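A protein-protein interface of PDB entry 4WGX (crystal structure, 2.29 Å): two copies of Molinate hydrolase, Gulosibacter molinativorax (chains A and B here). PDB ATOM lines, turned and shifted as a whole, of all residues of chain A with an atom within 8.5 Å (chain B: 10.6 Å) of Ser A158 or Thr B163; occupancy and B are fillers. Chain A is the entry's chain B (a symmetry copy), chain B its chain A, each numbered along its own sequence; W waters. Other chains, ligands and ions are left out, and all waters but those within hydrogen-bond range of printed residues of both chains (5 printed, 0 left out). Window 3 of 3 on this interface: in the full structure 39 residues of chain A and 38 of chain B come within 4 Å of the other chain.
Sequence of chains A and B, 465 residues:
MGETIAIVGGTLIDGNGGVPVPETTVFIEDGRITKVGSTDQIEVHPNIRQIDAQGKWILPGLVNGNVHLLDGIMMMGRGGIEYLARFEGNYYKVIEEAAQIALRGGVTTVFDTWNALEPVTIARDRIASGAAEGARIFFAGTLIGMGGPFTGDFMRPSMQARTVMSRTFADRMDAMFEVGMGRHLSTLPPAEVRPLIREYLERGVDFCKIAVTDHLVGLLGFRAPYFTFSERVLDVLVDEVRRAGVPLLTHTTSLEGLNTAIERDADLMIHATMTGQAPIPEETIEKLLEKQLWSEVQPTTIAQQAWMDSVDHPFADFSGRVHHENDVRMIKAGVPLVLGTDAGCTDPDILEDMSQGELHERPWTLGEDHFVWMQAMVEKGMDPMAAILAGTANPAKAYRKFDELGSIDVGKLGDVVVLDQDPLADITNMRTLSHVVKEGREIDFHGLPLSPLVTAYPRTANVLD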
ATOM      1  N   MET A  76     -21.261  12.510  26.303  1.00  0.00           N
ATOM      2  CA  MET A  76     -20.220  13.410  26.732  1.00  0.00           C
ATOM      3  C   MET A  76     -20.402  14.798  26.151  1.00  0.00           C
ATOM      4  O   MET A  76     -19.619  15.696  26.438  1.00  0.00           O
ATOM      5  CB  MET A  76     -18.855  12.853  26.357  1.00  0.00           C
ATOM      6  CG  MET A  76     -18.245  12.070  27.485  1.00  0.00           C
ATOM      7  SD  MET A  76     -16.469  12.081  27.377  1.00  0.00           S
ATOM      8  CE  MET A  76     -16.307  10.926  26.029  1.00  0.00           C
ATOM      9  N   GLY A  77     -21.441  14.973  25.348  1.00  0.00           N
ATOM     10  CA  GLY A  77     -21.862  16.298  24.934  1.00  0.00           C
ATOM     11  C   GLY A  77     -23.357  16.500  25.047  1.00  0.00           C
ATOM     12  O   GLY A  77     -23.970  16.245  26.076  1.00  0.00           O
ATOM     13  N   ARG A  78     -23.939  16.961  23.960  1.00  0.00           N
ATOM     14  CA  ARG A  78     -25.360  17.196  23.899  1.00  0.00           C
ATOM     15  C   ARG A  78     -26.062  15.895  23.529  1.00  0.00           C
ATOM     16  O   ARG A  78     -25.532  15.120  22.738  1.00  0.00           O
ATOM     17  CB  ARG A  78     -25.639  18.310  22.892  1.00  0.00           C
ATOM     18  CG  ARG A  78     -25.001  19.631  23.298  1.00  0.00           C
ATOM     19  CD  ARG A  78     -25.235  20.761  22.303  1.00  0.00           C
ATOM     20  NE  ARG A  78     -25.494  20.288  20.951  1.00  0.00           N
ATOM     21  CZ  ARG A  78     -24.555  20.027  20.044  1.00  0.00           C
ATOM     22  NH1 ARG A  78     -23.267  20.192  20.337  1.00  0.00           N
ATOM     23  NH2 ARG A  78     -24.904  19.598  18.833  1.00  0.00           N
ATOM     24  N   GLY A  79     -27.211  15.633  24.148  1.00  0.00           N
ATOM     25  CA  GLY A  79     -28.096  14.560  23.724  1.00  0.00           C
ATOM     26  C   GLY A  79     -28.365  13.431  24.706  1.00  0.00           C
ATOM     27  O   GLY A  79     -29.256  12.624  24.479  1.00  0.00           O
ATOM     28  N   ILE A  81     -29.755  13.292  27.775  1.00  0.00           N
ATOM     29  CA  ILE A  81     -31.070  13.276  28.401  1.00  0.00           C
ATOM     30  C   ILE A  81     -32.140  12.791  27.431  1.00  0.00           C
ATOM     31  O   ILE A  81     -32.920  11.908  27.758  1.00  0.00           O
ATOM     32  CB  ILE A  81     -31.489  14.660  28.918  1.00  0.00           C
ATOM     33  CG1 ILE A  81     -30.517  15.182  29.970  1.00  0.00           C
ATOM     34  CG2 ILE A  81     -32.877  14.592  29.551  1.00  0.00           C
ATOM     35  CD1 ILE A  81     -30.640  16.675  30.200  1.00  0.00           C
ATOM     36  N   GLU A  82     -32.176  13.378  26.242  1.00  0.00           N
ATOM     37  CA  GLU A  82     -33.232  13.091  25.285  1.00  0.00           C
ATOM     38  C   GLU A  82     -33.146  11.629  24.837  1.00  0.00           C
ATOM     39  O   GLU A  82     -34.147  10.918  24.796  1.00  0.00           O
ATOM     40  CB  GLU A  82     -33.172  14.077  24.098  1.00  0.00           C
ATOM     41  CG  GLU A  82     -31.984  13.994  23.162  1.00  0.00           C
ATOM     42  CD  GLU A  82     -31.745  15.309  22.393  1.00  0.00           C
ATOM     43  OE1 GLU A  82     -31.254  16.278  23.005  1.00  0.00           O
ATOM     44  OE2 GLU A  82     -32.055  15.385  21.184  1.00  0.00           O
ATOM     45  N   PHE A 154     -18.886  13.338  32.776  1.00  0.00           N
ATOM     46  CA  PHE A 154     -19.473  13.660  31.480  1.00  0.00           C
ATOM     47  C   PHE A 154     -19.835  15.136  31.380  1.00  0.00           C
ATOM     48  O   PHE A 154     -20.333  15.575  30.361  1.00  0.00           O
ATOM     49  CB  PHE A 154     -20.704  12.788  31.226  1.00  0.00           C
ATOM     50  CG  PHE A 154     -20.386  11.334  31.036  1.00  0.00           C
ATOM     51  CD1 PHE A 154     -20.077  10.532  32.120  1.00  0.00           C
ATOM     52  CD2 PHE A 154     -20.383  10.774  29.777  1.00  0.00           C
ATOM     53  CE1 PHE A 154     -19.782   9.190  31.951  1.00  0.00           C
ATOM     54  CE2 PHE A 154     -20.090   9.437  29.599  1.00  0.00           C
ATOM     55  CZ  PHE A 154     -19.780   8.642  30.691  1.00  0.00           C
ATOM     56  N   MET A 155     -19.568  15.907  32.427  1.00  0.00           N
ATOM     57  CA  MET A 155     -19.777  17.348  32.381  1.00  0.00           C
ATOM     58  C   MET A 155     -18.761  18.108  31.541  1.00  0.00           C
ATOM     59  O   MET A 155     -17.622  17.698  31.387  1.00  0.00           O
ATOM     60  CB  MET A 155     -19.724  17.951  33.774  1.00  0.00           C
ATOM     61  CG  MET A 155     -20.948  17.749  34.607  1.00  0.00           C
ATOM     62  SD  MET A 155     -20.788  18.503  36.230  1.00  0.00           S
ATOM     63  CE  MET A 155     -19.956  20.044  35.862  1.00  0.00           C
ATOM     64  N   ARG A 156     -19.207  19.238  31.016  1.00  0.00           N
ATOM     65  CA  ARG A 156     -18.325  20.278  30.530  1.00  0.00           C
ATOM     66  C   ARG A 156     -18.698  21.542  31.276  1.00  0.00           C
ATOM     67  O   ARG A 156     -19.780  21.624  31.838  1.00  0.00           O
ATOM     68  CB  ARG A 156     -18.454  20.468  29.034  1.00  0.00           C
ATOM     69  CG  ARG A 156     -18.234  19.207  28.278  1.00  0.00           C
ATOM     70  CD  ARG A 156     -17.917  19.497  26.860  1.00  0.00           C
ATOM     71  NE  ARG A 156     -18.268  18.377  26.010  1.00  0.00           N
ATOM     72  CZ  ARG A 156     -18.409  18.461  24.697  1.00  0.00           C
ATOM     73  NH1 ARG A 156     -18.230  19.622  24.083  1.00  0.00           N
ATOM     74  NH2 ARG A 156     -18.731  17.380  24.003  1.00  0.00           N
ATOM     75  N   PRO A 157     -17.804  22.533  31.300  1.00  0.00           N
ATOM     76  CA  PRO A 157     -18.089  23.733  32.086  1.00  0.00           C
ATOM     77  C   PRO A 157     -19.408  24.400  31.698  1.00  0.00           C
ATOM     78  O   PRO A 157     -20.087  24.945  32.558  1.00  0.00           O
ATOM     79  CB  PRO A 157     -16.892  24.631  31.779  1.00  0.00           C
ATOM     80  CG  PRO A 157     -15.813  23.682  31.395  1.00  0.00           C
ATOM     81  CD  PRO A 157     -16.511  22.635  30.609  1.00  0.00           C
ATOM     82  N   SER A 158     -19.784  24.315  30.426  1.00  0.00           N
ATOM     83  CA  SER A 158     -21.055  24.857  29.960  1.00  0.00           C
ATOM     84  C   SER A 158     -22.055  23.756  29.562  1.00  0.00           C
ATOM     85  O   SER A 158     -22.982  24.020  28.808  1.00  0.00           O
ATOM     86  CB  SER A 158     -20.820  25.810  28.779  1.00  0.00           C
ATOM     87  OG  SER A 158     -20.503  27.118  29.219  1.00  0.00           O
ATOM     88  N   MET A 159     -21.874  22.541  30.080  1.00  0.00           N
ATOM     89  CA  MET A 159     -22.821  21.448  29.860  1.00  0.00           C
ATOM     90  C   MET A 159     -23.048  20.648  31.115  1.00  0.00           C
ATOM     91  O   MET A 159     -22.307  19.718  31.400  1.00  0.00           O
ATOM     92  CB  MET A 159     -22.338  20.502  28.772  1.00  0.00           C
ATOM     93  CG  MET A 159     -22.132  21.170  27.450  1.00  0.00           C
ATOM     94  SD  MET A 159     -21.918  19.947  26.154  1.00  0.00           S
ATOM     95  CE  MET A 159     -21.090  20.935  24.933  1.00  0.00           C
ATOM     96  N   GLN A 160     -24.098  21.001  31.840  1.00  0.00           N
ATOM     97  CA  GLN A 160     -24.424  20.347  33.088  1.00  0.00           C
ATOM     98  C   GLN A 160     -25.869  19.893  33.029  1.00  0.00           C
ATOM     99  O   GLN A 160     -26.788  20.626  33.389  1.00  0.00           O
ATOM    100  CB  GLN A 160     -24.174  21.288  34.261  1.00  0.00           C
ATOM    101  CG  GLN A 160     -22.874  22.023  34.121  1.00  0.00           C
ATOM    102  CD  GLN A 160     -22.623  23.006  35.231  1.00  0.00           C
ATOM    103  OE1 GLN A 160     -23.290  22.992  36.267  1.00  0.00           O
ATOM    104  NE2 GLN A 160     -21.656  23.879  35.016  1.00  0.00           N
ATOM    105  N   ALA A 161     -26.043  18.673  32.539  1.00  0.00           N
ATOM    106  CA  ALA A 161     -27.352  18.082  32.330  1.00  0.00           C
ATOM    107  C   ALA A 161     -28.221  18.160  33.586  1.00  0.00           C
ATOM    108  O   ALA A 161     -29.407  18.439  33.505  1.00  0.00           O
ATOM    109  CB  ALA A 161     -27.193  16.638  31.883  1.00  0.00           C
ATOM    110  N   THR A 163     -28.588  20.277  35.765  1.00  0.00           N
ATOM    111  CA  THR A 163     -29.218  21.563  36.006  1.00  0.00           C
ATOM    112  C   THR A 163     -30.576  21.673  35.327  1.00  0.00           C
ATOM    113  O   THR A 163     -31.334  22.573  35.659  1.00  0.00           O
ATOM    114  CB  THR A 163     -28.353  22.769  35.522  1.00  0.00           C
ATOM    115  OG1 THR A 163     -28.178  22.723  34.101  1.00  0.00           O
ATOM    116  CG2 THR A 163     -27.001  22.797  36.201  1.00  0.00           C
ATOM    117  N   VAL A 164     -30.884  20.784  34.384  1.00  0.00           N
ATOM    118  CA  VAL A 164     -32.147  20.896  33.654  1.00  0.00           C
ATOM    119  C   VAL A 164     -32.939  19.595  33.586  1.00  0.00           C
ATOM    120  O   VAL A 164     -33.809  19.439  32.743  1.00  0.00           O
ATOM    121  CB  VAL A 164     -31.904  21.416  32.220  1.00  0.00           C
ATOM    122  CG1 VAL A 164     -31.269  22.788  32.264  1.00  0.00           C
ATOM    123  CG2 VAL A 164     -31.043  20.471  31.441  1.00  0.00           C
ATOM    124  N   GLY A 218     -13.547  16.277  29.747  1.00  0.00           N
ATOM    125  CA  GLY A 218     -14.599  17.176  29.316  1.00  0.00           C
ATOM    126  C   GLY A 218     -14.668  18.413  30.183  1.00  0.00           C
ATOM    127  O   GLY A 218     -14.990  19.501  29.725  1.00  0.00           O
ATOM    128  N   LEU A 219     -14.342  18.231  31.449  1.00  0.00           N
ATOM    129  CA  LEU A 219     -14.408  19.294  32.431  1.00  0.00           C
ATOM    130  C   LEU A 219     -13.117  20.113  32.559  1.00  0.00           C
ATOM    131  O   LEU A 219     -13.166  21.311  32.818  1.00  0.00           O
ATOM    132  CB  LEU A 219     -14.762  18.674  33.773  1.00  0.00           C
ATOM    133  CG  LEU A 219     -15.415  19.488  34.877  1.00  0.00           C
ATOM    134  CD1 LEU A 219     -16.527  20.389  34.373  1.00  0.00           C
ATOM    135  CD2 LEU A 219     -15.952  18.500  35.869  1.00  0.00           C
ATOM    136  N   ILE B  81     -36.839  18.542  28.700  1.00  0.00           N
ATOM    137  CA  ILE B  81     -36.224  17.685  27.696  1.00  0.00           C
ATOM    138  C   ILE B  81     -36.693  16.245  27.844  1.00  0.00           C
ATOM    139  O   ILE B  81     -37.072  15.601  26.873  1.00  0.00           O
ATOM    140  CB  ILE B  81     -34.680  17.688  27.770  1.00  0.00           C
ATOM    141  CG1 ILE B  81     -34.128  19.088  27.552  1.00  0.00           C
ATOM    142  CG2 ILE B  81     -34.098  16.763  26.713  1.00  0.00           C
ATOM    143  CD1 ILE B  81     -32.680  19.246  27.966  1.00  0.00           C
ATOM    144  N   PRO B 149     -40.506  26.382  24.409  1.00  0.00           N
ATOM    145  CA  PRO B 149     -39.924  25.931  25.675  1.00  0.00           C
ATOM    146  C   PRO B 149     -38.385  25.880  25.713  1.00  0.00           C
ATOM    147  O   PRO B 149     -37.821  25.696  26.783  1.00  0.00           O
ATOM    148  CB  PRO B 149     -40.513  24.529  25.839  1.00  0.00           C
ATOM    149  CG  PRO B 149     -40.809  24.076  24.484  1.00  0.00           C
ATOM    150  CD  PRO B 149     -41.203  25.292  23.711  1.00  0.00           C
ATOM    151  N   PHE B 150     -37.729  26.043  24.575  1.00  0.00           N
ATOM    152  CA  PHE B 150     -36.273  26.056  24.521  1.00  0.00           C
ATOM    153  C   PHE B 150     -35.740  27.376  23.992  1.00  0.00           C
ATOM    154  O   PHE B 150     -34.741  27.431  23.305  1.00  0.00           O
ATOM    155  CB  PHE B 150     -35.794  24.860  23.701  1.00  0.00           C
ATOM    156  CG  PHE B 150     -36.259  23.565  24.284  1.00  0.00           C
ATOM    157  CD1 PHE B 150     -35.815  23.177  25.527  1.00  0.00           C
ATOM    158  CD2 PHE B 150     -37.207  22.785  23.650  1.00  0.00           C
ATOM    159  CE1 PHE B 150     -36.266  22.025  26.105  1.00  0.00           C
ATOM    160  CE2 PHE B 150     -37.655  21.627  24.230  1.00  0.00           C
ATOM    161  CZ  PHE B 150     -37.190  21.252  25.456  1.00  0.00           C
ATOM    162  N   THR B 151     -36.414  28.448  24.377  1.00  0.00           N
ATOM    163  CA  THR B 151     -35.970  29.804  24.093  1.00  0.00           C
ATOM    164  C   THR B 151     -35.738  30.505  25.418  1.00  0.00           C
ATOM    165  O   THR B 151     -35.802  29.871  26.462  1.00  0.00           O
ATOM    166  CB  THR B 151     -36.999  30.575  23.268  1.00  0.00           C
ATOM    167  OG1 THR B 151     -38.168  30.823  24.058  1.00  0.00           O
ATOM    168  CG2 THR B 151     -37.368  29.795  22.038  1.00  0.00           C
ATOM    169  N   MET B 155     -35.755  29.896  29.979  1.00  0.00           N
ATOM    170  CA  MET B 155     -34.418  29.827  30.564  1.00  0.00           C
ATOM    171  C   MET B 155     -34.330  30.407  31.958  1.00  0.00           C
ATOM    172  O   MET B 155     -35.089  31.286  32.331  1.00  0.00           O
ATOM    173  CB  MET B 155     -33.404  30.581  29.718  1.00  0.00           C
ATOM    174  CG  MET B 155     -32.911  29.857  28.513  1.00  0.00           C
ATOM    175  SD  MET B 155     -31.647  30.776  27.609  1.00  0.00           S
ATOM    176  CE  MET B 155     -30.970  31.885  28.829  1.00  0.00           C
ATOM    177  N   ARG B 156     -33.380  29.899  32.720  1.00  0.00           N
ATOM    178  CA  ARG B 156     -32.910  30.576  33.919  1.00  0.00           C
ATOM    179  C   ARG B 156     -31.410  30.723  33.806  1.00  0.00           C
ATOM    180  O   ARG B 156     -30.797  30.102  32.946  1.00  0.00           O
ATOM    181  CB  ARG B 156     -33.276  29.813  35.178  1.00  0.00           C
ATOM    182  CG  ARG B 156     -34.708  29.427  35.225  1.00  0.00           C
ATOM    183  CD  ARG B 156     -35.151  29.298  36.641  1.00  0.00           C
ATOM    184  NE  ARG B 156     -36.282  28.403  36.757  1.00  0.00           N
ATOM    185  CZ  ARG B 156     -36.651  27.812  37.884  1.00  0.00           C
ATOM    186  NH1 ARG B 156     -35.964  28.020  39.000  1.00  0.00           N
ATOM    187  NH2 ARG B 156     -37.701  27.003  37.893  1.00  0.00           N
ATOM    188  N   PRO B 157     -30.812  31.546  34.670  1.00  0.00           N
ATOM    189  CA  PRO B 157     -29.381  31.801  34.517  1.00  0.00           C
ATOM    190  C   PRO B 157     -28.563  30.513  34.613  1.00  0.00           C
ATOM    191  O   PRO B 157     -27.620  30.359  33.847  1.00  0.00           O
ATOM    192  CB  PRO B 157     -29.087  32.783  35.653  1.00  0.00           C
ATOM    193  CG  PRO B 157     -30.415  33.425  35.921  1.00  0.00           C
ATOM    194  CD  PRO B 157     -31.376  32.311  35.791  1.00  0.00           C
ATOM    195  N   SER B 158     -28.968  29.610  35.511  1.00  0.00           N
ATOM    196  CA  SER B 158     -28.316  28.307  35.694  1.00  0.00           C
ATOM    197  C   SER B 158     -29.023  27.143  34.992  1.00  0.00           C
ATOM    198  O   SER B 158     -28.667  25.993  35.216  1.00  0.00           O
ATOM    199  CB  SER B 158     -28.215  27.963  37.184  1.00  0.00           C
ATOM    200  OG  SER B 158     -29.398  27.335  37.642  1.00  0.00           O
ATOM    201  N   MET B 159     -30.021  27.429  34.160  1.00  0.00           N
ATOM    202  CA  MET B 159     -30.785  26.371  33.475  1.00  0.00           C
ATOM    203  C   MET B 159     -30.986  26.710  32.015  1.00  0.00           C
ATOM    204  O   MET B 159     -31.888  27.465  31.666  1.00  0.00           O
ATOM    205  CB  MET B 159     -32.152  26.146  34.110  1.00  0.00           C
ATOM    206  CG  MET B 159     -32.135  25.912  35.592  1.00  0.00           C
ATOM    207  SD  MET B 159     -33.774  25.413  36.141  1.00  0.00           S
ATOM    208  CE  MET B 159     -33.488  25.293  37.898  1.00  0.00           C
ATOM    209  N   GLN B 160     -30.143  26.140  31.168  1.00  0.00           N
ATOM    210  CA  GLN B 160     -30.187  26.414  29.745  1.00  0.00           C
ATOM    211  C   GLN B 160     -30.191  25.096  29.005  1.00  0.00           C
ATOM    212  O   GLN B 160     -29.141  24.519  28.746  1.00  0.00           O
ATOM    213  CB  GLN B 160     -29.006  27.283  29.322  1.00  0.00           C
ATOM    214  CG  GLN B 160     -28.793  28.479  30.219  1.00  0.00           C
ATOM    215  CD  GLN B 160     -27.579  29.279  29.841  1.00  0.00           C
ATOM    216  OE1 GLN B 160     -27.069  29.168  28.731  1.00  0.00           O
ATOM    217  NE2 GLN B 160     -27.096  30.086  30.769  1.00  0.00           N
ATOM    218  N   ALA B 161     -31.388  24.630  28.667  1.00  0.00           N
ATOM    219  CA  ALA B 161     -31.575  23.300  28.100  1.00  0.00           C
ATOM    220  C   ALA B 161     -30.809  23.132  26.801  1.00  0.00           C
ATOM    221  O   ALA B 161     -30.235  22.085  26.536  1.00  0.00           O
ATOM    222  CB  ALA B 161     -33.046  23.032  27.887  1.00  0.00           C
ATOM    223  N   ARG B 162     -30.766  24.186  26.004  1.00  0.00           N
ATOM    224  CA  ARG B 162     -30.120  24.104  24.710  1.00  0.00           C
ATOM    225  C   ARG B 162     -28.613  23.824  24.791  1.00  0.00           C
ATOM    226  O   ARG B 162     -28.017  23.379  23.816  1.00  0.00           O
ATOM    227  CB  ARG B 162     -30.407  25.377  23.914  1.00  0.00           C
ATOM    228  CG  ARG B 162     -31.630  25.161  23.054  1.00  0.00           C
ATOM    229  CD  ARG B 162     -32.149  26.343  22.271  1.00  0.00           C
ATOM    230  NE  ARG B 162     -31.856  26.099  20.875  1.00  0.00           N
ATOM    231  CZ  ARG B 162     -32.749  25.864  19.925  1.00  0.00           C
ATOM    232  NH1 ARG B 162     -34.047  25.907  20.170  1.00  0.00           N
ATOM    233  NH2 ARG B 162     -32.325  25.609  18.704  1.00  0.00           N
ATOM    234  N   THR B 163     -28.004  24.023  25.955  1.00  0.00           N
ATOM    235  CA  THR B 163     -26.605  23.650  26.106  1.00  0.00           C
ATOM    236  C   THR B 163     -26.417  22.132  26.156  1.00  0.00           C
ATOM    237  O   THR B 163     -25.323  21.662  25.855  1.00  0.00           O
ATOM    238  CB  THR B 163     -25.954  24.261  27.370  1.00  0.00           C
ATOM    239  OG1 THR B 163     -26.567  23.728  28.546  1.00  0.00           O
ATOM    240  CG2 THR B 163     -26.063  25.779  27.365  1.00  0.00           C
ATOM    241  N   VAL B 164     -27.457  21.371  26.509  1.00  0.00           N
ATOM    242  CA  VAL B 164     -27.291  19.922  26.637  1.00  0.00           C
ATOM    243  C   VAL B 164     -28.256  19.077  25.787  1.00  0.00           C
ATOM    244  O   VAL B 164     -28.460  17.899  26.060  1.00  0.00           O
ATOM    245  CB  VAL B 164     -27.436  19.479  28.102  1.00  0.00           C
ATOM    246  CG1 VAL B 164     -26.329  20.069  28.947  1.00  0.00           C
ATOM    247  CG2 VAL B 164     -28.794  19.855  28.647  1.00  0.00           C
ATOM    248  N   MET B 165     -28.820  19.664  24.743  1.00  0.00           N
ATOM    249  CA  MET B 165     -29.706  18.927  23.852  1.00  0.00           C
ATOM    250  C   MET B 165     -29.345  19.220  22.412  1.00  0.00           C
ATOM    251  O   MET B 165     -28.634  20.175  22.124  1.00  0.00           O
ATOM    252  CB  MET B 165     -31.164  19.286  24.129  1.00  0.00           C
ATOM    253  CG  MET B 165     -31.523  20.708  23.788  1.00  0.00           C
ATOM    254  SD  MET B 165     -33.111  21.235  24.452  1.00  0.00           S
ATOM    255  CE  MET B 165     -34.211  20.161  23.542  1.00  0.00           C
ATOM    256  N   SER B 166     -29.806  18.371  21.507  1.00  0.00           N
ATOM    257  CA  SER B 166     -29.583  18.594  20.089  1.00  0.00           C
ATOM    258  C   SER B 166     -30.344  19.833  19.664  1.00  0.00           C
ATOM    259  O   SER B 166     -31.448  20.069  20.133  1.00  0.00           O
ATOM    260  CB  SER B 166     -30.040  17.394  19.263  1.00  0.00           C
ATOM    261  OG  SER B 166     -31.441  17.234  19.340  1.00  0.00           O
ATOM    262  N   ARG B 167     -29.754  20.620  18.779  1.00  0.00           N
ATOM    263  CA  ARG B 167     -30.426  21.781  18.233  1.00  0.00           C
ATOM    264  C   ARG B 167     -31.668  21.353  17.448  1.00  0.00           C
ATOM    265  O   ARG B 167     -32.697  22.021  17.456  1.00  0.00           O
ATOM    266  CB  ARG B 167     -29.467  22.566  17.343  1.00  0.00           C
ATOM    267  CG  ARG B 167     -30.072  23.824  16.742  1.00  0.00           C
ATOM    268  CD  ARG B 167     -29.094  24.532  15.838  1.00  0.00           C
ATOM    269  NE  ARG B 167     -28.780  23.731  14.659  1.00  0.00           N
ATOM    270  CZ  ARG B 167     -27.634  23.080  14.455  1.00  0.00           C
ATOM    271  NH1 ARG B 167     -26.642  23.129  15.345  1.00  0.00           N
ATOM    272  NH2 ARG B 167     -27.476  22.379  13.341  1.00  0.00           N
ATOM    273  N   THR B 168     -31.548  20.221  16.764  1.00  0.00           N
ATOM    274  CA  THR B 168     -32.613  19.704  15.911  1.00  0.00           C
ATOM    275  C   THR B 168     -33.888  19.420  16.710  1.00  0.00           C
ATOM    276  O   THR B 168     -34.983  19.891  16.357  1.00  0.00           O
ATOM    277  CB  THR B 168     -32.128  18.430  15.180  1.00  0.00           C
ATOM    278  OG1 THR B 168     -31.042  18.776  14.315  1.00  0.00           O
ATOM    279  CG2 THR B 168     -33.225  17.790  14.355  1.00  0.00           C
ATOM    280  N   ALA B 170     -34.579  20.510  19.799  1.00  0.00           N
ATOM    281  CA  ALA B 170     -35.009  21.758  20.422  1.00  0.00           C
ATOM    282  C   ALA B 170     -35.821  22.579  19.436  1.00  0.00           C
ATOM    283  O   ALA B 170     -36.874  23.103  19.781  1.00  0.00           O
ATOM    284  CB  ALA B 170     -33.808  22.561  20.933  1.00  0.00           C
HETATM  285  O   HOH W   1     -27.987  15.841  27.841  1.00  0.00           O
HETATM  286  O   HOH W   2     -35.102  20.440  30.529  1.00  0.00           O
HETATM  287  O   HOH W   3     -30.700  15.949  25.588  1.00  0.00           O
HETATM  288  O   HOH W   4     -25.606  23.436  31.066  1.00  0.00           O
HETATM  289  O   HOH W   5     -27.776  24.601  32.337  1.00  0.00           O
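The side-chain hydroxyl of Thr B163 sits at hydrogen-bond distance from the backbone carbonyl oxygen of Gln B160. O of Pro A157 sits at hydrogen-bond distance from NE2 of Gln A160 (3.1 Å). The backbone carbonyl oxygen of Pro B157 is in hydrogen-bond range of the side-chain amide nitrogen of Gln B160, at 3.1 Å. The side-chain hydroxyl (OG1) of Thr A163 is in hydrogen-bond range of the backbone carbonyl oxygen (O) of Gln A160, at 2.6 Å.
Of the 19 printed residues of chain B, 8 touch a printed residue of chain A. Among the printed residues, 19 pairs touch across the chains. Among the printed residues, no Asp or Glu carboxylate lies within 4 Å of a Lys or Arg side-chain nitrogen of the other chain.
Printed residues of chain B within 4 Å of Gly A79: Val B164. Of the printed residues of chain B, Ile A81 touches Ile B81 and Val B164. No residue of chain B comes within 4 Å of Pro A157. Ser A158 touches one residue of chain B. Printed residues of chain B within 4 Å of Ala A161: Val B164. Printed residues of chain A within 4 Å of Gln B160: Val A164. Of chain A, only Arg A78, Ser A158 and Met A159 come within 4 Å of Thr B163. Ala B170 touches none of the printed residues of chain A. The nearest residue of chain B that does not touch Ser A158 is Val B164 (5.2 Å).
O of Thr A163 lies close to SD of Met B159. The backbone carbonyl oxygen (O) of Val B164 lies within hydrogen-bond range of the backbone NH (N) of Gly A79. OG1 of Thr A163 lies close to O of Ser B158. The side-chain hydroxyl (OG) of Ser B166 is in hydrogen-bond range of the side-chain carboxylate (OE2) of Glu A82 (2.7 Å). O of Met B165 sits at hydrogen-bond distance from NE of Arg A78, at 3.4 Å.
Water W5 lies within hydrogen-bond range of the side-chain hydroxyl (OG1) of Thr A163 (2.6 Å), the backbone NH (N) of Gln B160 (3.1 Å) and the backbone carbonyl oxygen (O) of Ser B158 (3.3 Å). Water W3 lies within hydrogen-bond range of OE1 of Glu A82 (2.7 Å) and O of Val B164 (3.0 Å). Water W4 lies within hydrogen-bond range of OG1 of Thr B163 (2.7 Å) and N of Gln A160 (3.0 Å). Water W2 bridges the backbone carbonyl oxygen (O) of Val A164 (2.8 Å) and the backbone NH (N) of Ile B81 (3.2 Å). Water W1 lies within hydrogen-bond range of O of Val B164 (2.8 Å) and N of Ile A81 (3.1 Å).
Ser A158 touches Thr B163, and with the chains exchanged Thr A163 touches Ser B158. Met A159 touches Thr B163, and with the chains exchanged Thr A163 touches Met B159. Met A159 touches Val B164, and with the chains exchanged Val A164 touches Met B159. Gln A160 touches Val B164, and with the chains exchanged Val A164 touches Gln B160. Of the 19 pairs that touch across the chains among the printed residues, 10 have their exchanged pair printed and touching as well.
Among the printed residues, merely in contact across the chains: Glu A82 with Met B165 (3.2 Å), Arg A78 with Thr B163 (3.3 Å), Ser A158 with Thr B163 (3.3 Å), Met A159 with Thr B163 (3.6 Å), Val A164 with Val B164 (3.6 Å), Val A164 with Gln B160 (3.7 Å), Gln A160 with Val B164 (3.8 Å), Ile A81 with Ile B81 (3.8 Å), Val A164 with Met B159 (3.8 Å), Arg A78 with Val B164 (3.8 Å), Glu A82 with Ile B81 (3.9 Å), Ala A161 with Val B164 (3.9 Å), Met A159 with Val B164 (3.9 Å) and Ile A81 with Val B164 (3.99 Å).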
